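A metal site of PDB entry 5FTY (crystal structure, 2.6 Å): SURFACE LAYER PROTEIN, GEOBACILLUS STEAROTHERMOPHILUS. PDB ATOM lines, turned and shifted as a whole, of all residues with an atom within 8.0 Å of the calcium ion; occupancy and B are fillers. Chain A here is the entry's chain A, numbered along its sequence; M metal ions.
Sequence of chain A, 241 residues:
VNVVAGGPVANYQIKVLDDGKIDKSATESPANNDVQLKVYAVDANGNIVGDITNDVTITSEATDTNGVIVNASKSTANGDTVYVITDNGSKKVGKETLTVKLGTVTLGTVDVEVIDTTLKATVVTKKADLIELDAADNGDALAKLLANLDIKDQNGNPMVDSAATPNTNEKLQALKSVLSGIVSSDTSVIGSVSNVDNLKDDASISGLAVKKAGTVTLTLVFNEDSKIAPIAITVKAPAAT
The backbone carbonyl oxygen (O) of Thr 168 sits close to the side-chain hydroxyl (OG1) of Thr 165.
The side-chain hydroxyl (OG1) of Thr 165 sits close to the side-chain carboxylate (OE2) of Glu 170 (2.5 Å).
OE1 of Glu 170 is in hydrogen-bond range of N of Ser 162, 2.8 Å away.
The side-chain carboxylate (OD1) of Asp 201 lies within hydrogen-bond range of the side-chain hydroxyl (OG1) of Thr 168 (3.1 Å).
Merely in contact with the calcium ion: Pro 166.
The nearest printed residue that does not touch the calcium ion is Glu 170 (4.2 Å).
O of Thr 165 is bound to the calcium ion, at 2.3 Å.
The calcium ion is bound by OD1 of Asp 161, 2.3 Å away.
O of Ser 162 binds the calcium ion, at 2.5 Å.
OG1 of Thr 165 binds the calcium ion (2.7 Å).
The calcium ion has four donor atoms within binding distance.
Slightly farther from the calcium ion lies the backbone carbonyl oxygen (O) of Thr 168 (3.0 Å).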
ATOM      1  N   VAL A 160     -27.032  -7.191  17.494  1.00  0.00           N
ATOM      2  CA  VAL A 160     -26.745  -5.807  17.872  1.00  0.00           C
ATOM      3  C   VAL A 160     -25.666  -5.729  18.958  1.00  0.00           C
ATOM      4  O   VAL A 160     -25.612  -6.581  19.842  1.00  0.00           O
ATOM      5  CB  VAL A 160     -28.038  -5.106  18.338  1.00  0.00           C
ATOM      6  CG1 VAL A 160     -27.756  -3.952  19.297  1.00  0.00           C
ATOM      7  CG2 VAL A 160     -28.857  -4.643  17.142  1.00  0.00           C
ATOM      8  N   ASP A 161     -24.812  -4.719  18.874  1.00  0.00           N
ATOM      9  CA  ASP A 161     -23.857  -4.423  19.930  1.00  0.00           C
ATOM     10  C   ASP A 161     -24.571  -4.036  21.225  1.00  0.00           C
ATOM     11  O   ASP A 161     -25.270  -3.032  21.281  1.00  0.00           O
ATOM     12  CB  ASP A 161     -22.911  -3.293  19.499  1.00  0.00           C
ATOM     13  CG  ASP A 161     -21.818  -3.037  20.513  1.00  0.00           C
ATOM     14  OD1 ASP A 161     -21.497  -3.961  21.285  1.00  0.00           O
ATOM     15  OD2 ASP A 161     -21.271  -1.908  20.543  1.00  0.00           O
ATOM     16  N   SER A 162     -24.389  -4.859  22.250  1.00  0.00           N
ATOM     17  CA  SER A 162     -25.009  -4.625  23.549  1.00  0.00           C
ATOM     18  C   SER A 162     -24.104  -3.740  24.408  1.00  0.00           C
ATOM     19  O   SER A 162     -22.894  -3.910  24.410  1.00  0.00           O
ATOM     20  CB  SER A 162     -25.270  -5.958  24.256  1.00  0.00           C
ATOM     21  OG  SER A 162     -25.992  -5.779  25.459  1.00  0.00           O
ATOM     22  N   ALA A 163     -24.710  -2.792  25.125  1.00  0.00           N
ATOM     23  CA  ALA A 163     -23.930  -1.823  25.899  1.00  0.00           C
ATOM     24  C   ALA A 163     -23.326  -2.444  27.156  1.00  0.00           C
ATOM     25  O   ALA A 163     -22.387  -1.893  27.733  1.00  0.00           O
ATOM     26  CB  ALA A 163     -24.786  -0.616  26.244  1.00  0.00           C
ATOM     27  N   ALA A 164     -23.876  -3.578  27.584  1.00  0.00           N
ATOM     28  CA  ALA A 164     -23.379  -4.252  28.776  1.00  0.00           C
ATOM     29  C   ALA A 164     -22.144  -5.089  28.484  1.00  0.00           C
ATOM     30  O   ALA A 164     -21.644  -5.811  29.343  1.00  0.00           O
ATOM     31  CB  ALA A 164     -24.474  -5.113  29.399  1.00  0.00           C
ATOM     32  N   THR A 165     -21.648  -5.010  27.244  1.00  0.00           N
ATOM     33  CA  THR A 165     -20.435  -5.702  26.872  1.00  0.00           C
ATOM     34  C   THR A 165     -19.473  -4.757  26.160  1.00  0.00           C
ATOM     35  O   THR A 165     -19.138  -4.970  24.999  1.00  0.00           O
ATOM     36  CB  THR A 165     -20.729  -6.887  25.919  1.00  0.00           C
ATOM     37  OG1 THR A 165     -20.735  -6.418  24.559  1.00  0.00           O
ATOM     38  CG2 THR A 165     -22.059  -7.546  26.243  1.00  0.00           C
ATOM     39  N   PRO A 166     -18.987  -3.728  26.876  1.00  0.00           N
ATOM     40  CA  PRO A 166     -18.217  -2.645  26.245  1.00  0.00           C
ATOM     41  C   PRO A 166     -16.883  -3.107  25.664  1.00  0.00           C
ATOM     42  O   PRO A 166     -16.211  -2.327  24.987  1.00  0.00           O
ATOM     43  CB  PRO A 166     -17.970  -1.684  27.412  1.00  0.00           C
ATOM     44  CG  PRO A 166     -17.981  -2.546  28.610  1.00  0.00           C
ATOM     45  CD  PRO A 166     -19.012  -3.601  28.338  1.00  0.00           C
ATOM     46  N   ASN A 167     -16.511  -4.356  25.916  1.00  0.00           N
ATOM     47  CA  ASN A 167     -15.280  -4.915  25.384  1.00  0.00           C
ATOM     48  C   ASN A 167     -15.324  -5.072  23.865  1.00  0.00           C
ATOM     49  O   ASN A 167     -14.493  -4.511  23.147  1.00  0.00           O
ATOM     50  CB  ASN A 167     -15.000  -6.272  26.026  1.00  0.00           C
ATOM     51  CG  ASN A 167     -15.046  -6.214  27.546  1.00  0.00           C
ATOM     52  OD1 ASN A 167     -16.102  -5.948  28.134  1.00  0.00           O
ATOM     53  ND2 ASN A 167     -13.915  -6.478  28.180  1.00  0.00           N
ATOM     54  N   THR A 168     -16.316  -5.823  23.375  1.00  0.00           N
ATOM     55  CA  THR A 168     -16.392  -6.168  21.965  1.00  0.00           C
ATOM     56  C   THR A 168     -17.745  -5.833  21.353  1.00  0.00           C
ATOM     57  O   THR A 168     -18.774  -5.852  22.024  1.00  0.00           O
ATOM     58  CB  THR A 168     -16.075  -7.669  21.755  1.00  0.00           C
ATOM     59  OG1 THR A 168     -16.198  -7.987  20.366  1.00  0.00           O
ATOM     60  CG2 THR A 168     -17.043  -8.540  22.553  1.00  0.00           C
ATOM     61  N   ASN A 169     -17.741  -5.531  20.056  1.00  0.00           N
ATOM     62  CA  ASN A 169     -18.959  -5.252  19.299  1.00  0.00           C
ATOM     63  C   ASN A 169     -19.563  -6.562  18.796  1.00  0.00           C
ATOM     64  O   ASN A 169     -18.949  -7.254  17.979  1.00  0.00           O
ATOM     65  CB  ASN A 169     -18.644  -4.321  18.130  1.00  0.00           C
ATOM     66  CG  ASN A 169     -19.891  -3.778  17.458  1.00  0.00           C
ATOM     67  OD1 ASN A 169     -20.798  -4.525  17.111  1.00  0.00           O
ATOM     68  ND2 ASN A 169     -19.936  -2.465  17.279  1.00  0.00           N
ATOM     69  N   GLU A 170     -20.752  -6.897  19.277  1.00  0.00           N
ATOM     70  CA  GLU A 170     -21.406  -8.146  18.882  1.00  0.00           C
ATOM     71  C   GLU A 170     -21.876  -8.117  17.429  1.00  0.00           C
ATOM     72  O   GLU A 170     -21.984  -9.157  16.790  1.00  0.00           O
ATOM     73  CB  GLU A 170     -22.601  -8.458  19.797  1.00  0.00           C
ATOM     74  CG  GLU A 170     -22.225  -9.178  21.086  1.00  0.00           C
ATOM     75  CD  GLU A 170     -22.143  -8.231  22.271  1.00  0.00           C
ATOM     76  OE1 GLU A 170     -22.982  -7.308  22.359  1.00  0.00           O
ATOM     77  OE2 GLU A 170     -21.239  -8.414  23.116  1.00  0.00           O
ATOM     78  N   LYS A 171     -22.145  -6.922  16.916  1.00  0.00           N
ATOM     79  CA  LYS A 171     -22.631  -6.759  15.553  1.00  0.00           C
ATOM     80  C   LYS A 171     -21.485  -6.899  14.551  1.00  0.00           C
ATOM     81  O   LYS A 171     -21.641  -7.533  13.506  1.00  0.00           O
ATOM     82  CB  LYS A 171     -23.348  -5.417  15.385  1.00  0.00           C
ATOM     83  CG  LYS A 171     -23.907  -5.191  13.997  1.00  0.00           C
ATOM     84  CD  LYS A 171     -24.657  -3.878  13.902  1.00  0.00           C
ATOM     85  CE  LYS A 171     -25.224  -3.674  12.511  1.00  0.00           C
ATOM     86  NZ  LYS A 171     -26.009  -2.415  12.388  1.00  0.00           N
ATOM     87  N   ASP A 201     -11.712  -4.975  16.714  1.00  0.00           N
ATOM     88  CA  ASP A 201     -12.811  -4.863  17.674  1.00  0.00           C
ATOM     89  C   ASP A 201     -12.423  -4.105  18.946  1.00  0.00           C
ATOM     90  O   ASP A 201     -11.709  -4.617  19.799  1.00  0.00           O
ATOM     91  CB  ASP A 201     -13.314  -6.267  18.049  1.00  0.00           C
ATOM     92  CG  ASP A 201     -14.815  -6.404  17.892  1.00  0.00           C
ATOM     93  OD1 ASP A 201     -15.553  -5.596  18.478  1.00  0.00           O
ATOM     94  OD2 ASP A 201     -15.250  -7.319  17.157  1.00  0.00           O
ATOM     95  N   ASP A 202     -12.914  -2.868  19.048  1.00  0.00           N
ATOM     96  CA  ASP A 202     -12.714  -2.031  20.226  1.00  0.00           C
ATOM     97  C   ASP A 202     -13.905  -1.088  20.361  1.00  0.00           C
ATOM     98  O   ASP A 202     -14.888  -1.218  19.636  1.00  0.00           O
ATOM     99  CB  ASP A 202     -11.429  -1.216  20.090  1.00  0.00           C
ATOM    100  CG  ASP A 202     -10.178  -2.007  20.431  1.00  0.00           C
ATOM    101  OD1 ASP A 202      -9.811  -2.050  21.621  1.00  0.00           O
ATOM    102  OD2 ASP A 202      -9.557  -2.583  19.505  1.00  0.00           O
ATOM    103  N   ALA A 203     -13.814  -0.144  21.282  1.00  0.00           N
ATOM    104  CA  ALA A 203     -14.831   0.904  21.380  1.00  0.00           C
ATOM    105  C   ALA A 203     -14.708   1.773  20.138  1.00  0.00           C
ATOM    106  O   ALA A 203     -15.700   2.235  19.582  1.00  0.00           O
ATOM    107  CB  ALA A 203     -14.647   1.723  22.640  1.00  0.00           C
HETATM  108 CA    CA M   1     -20.599  -3.992  23.456  1.00  0.00          CA
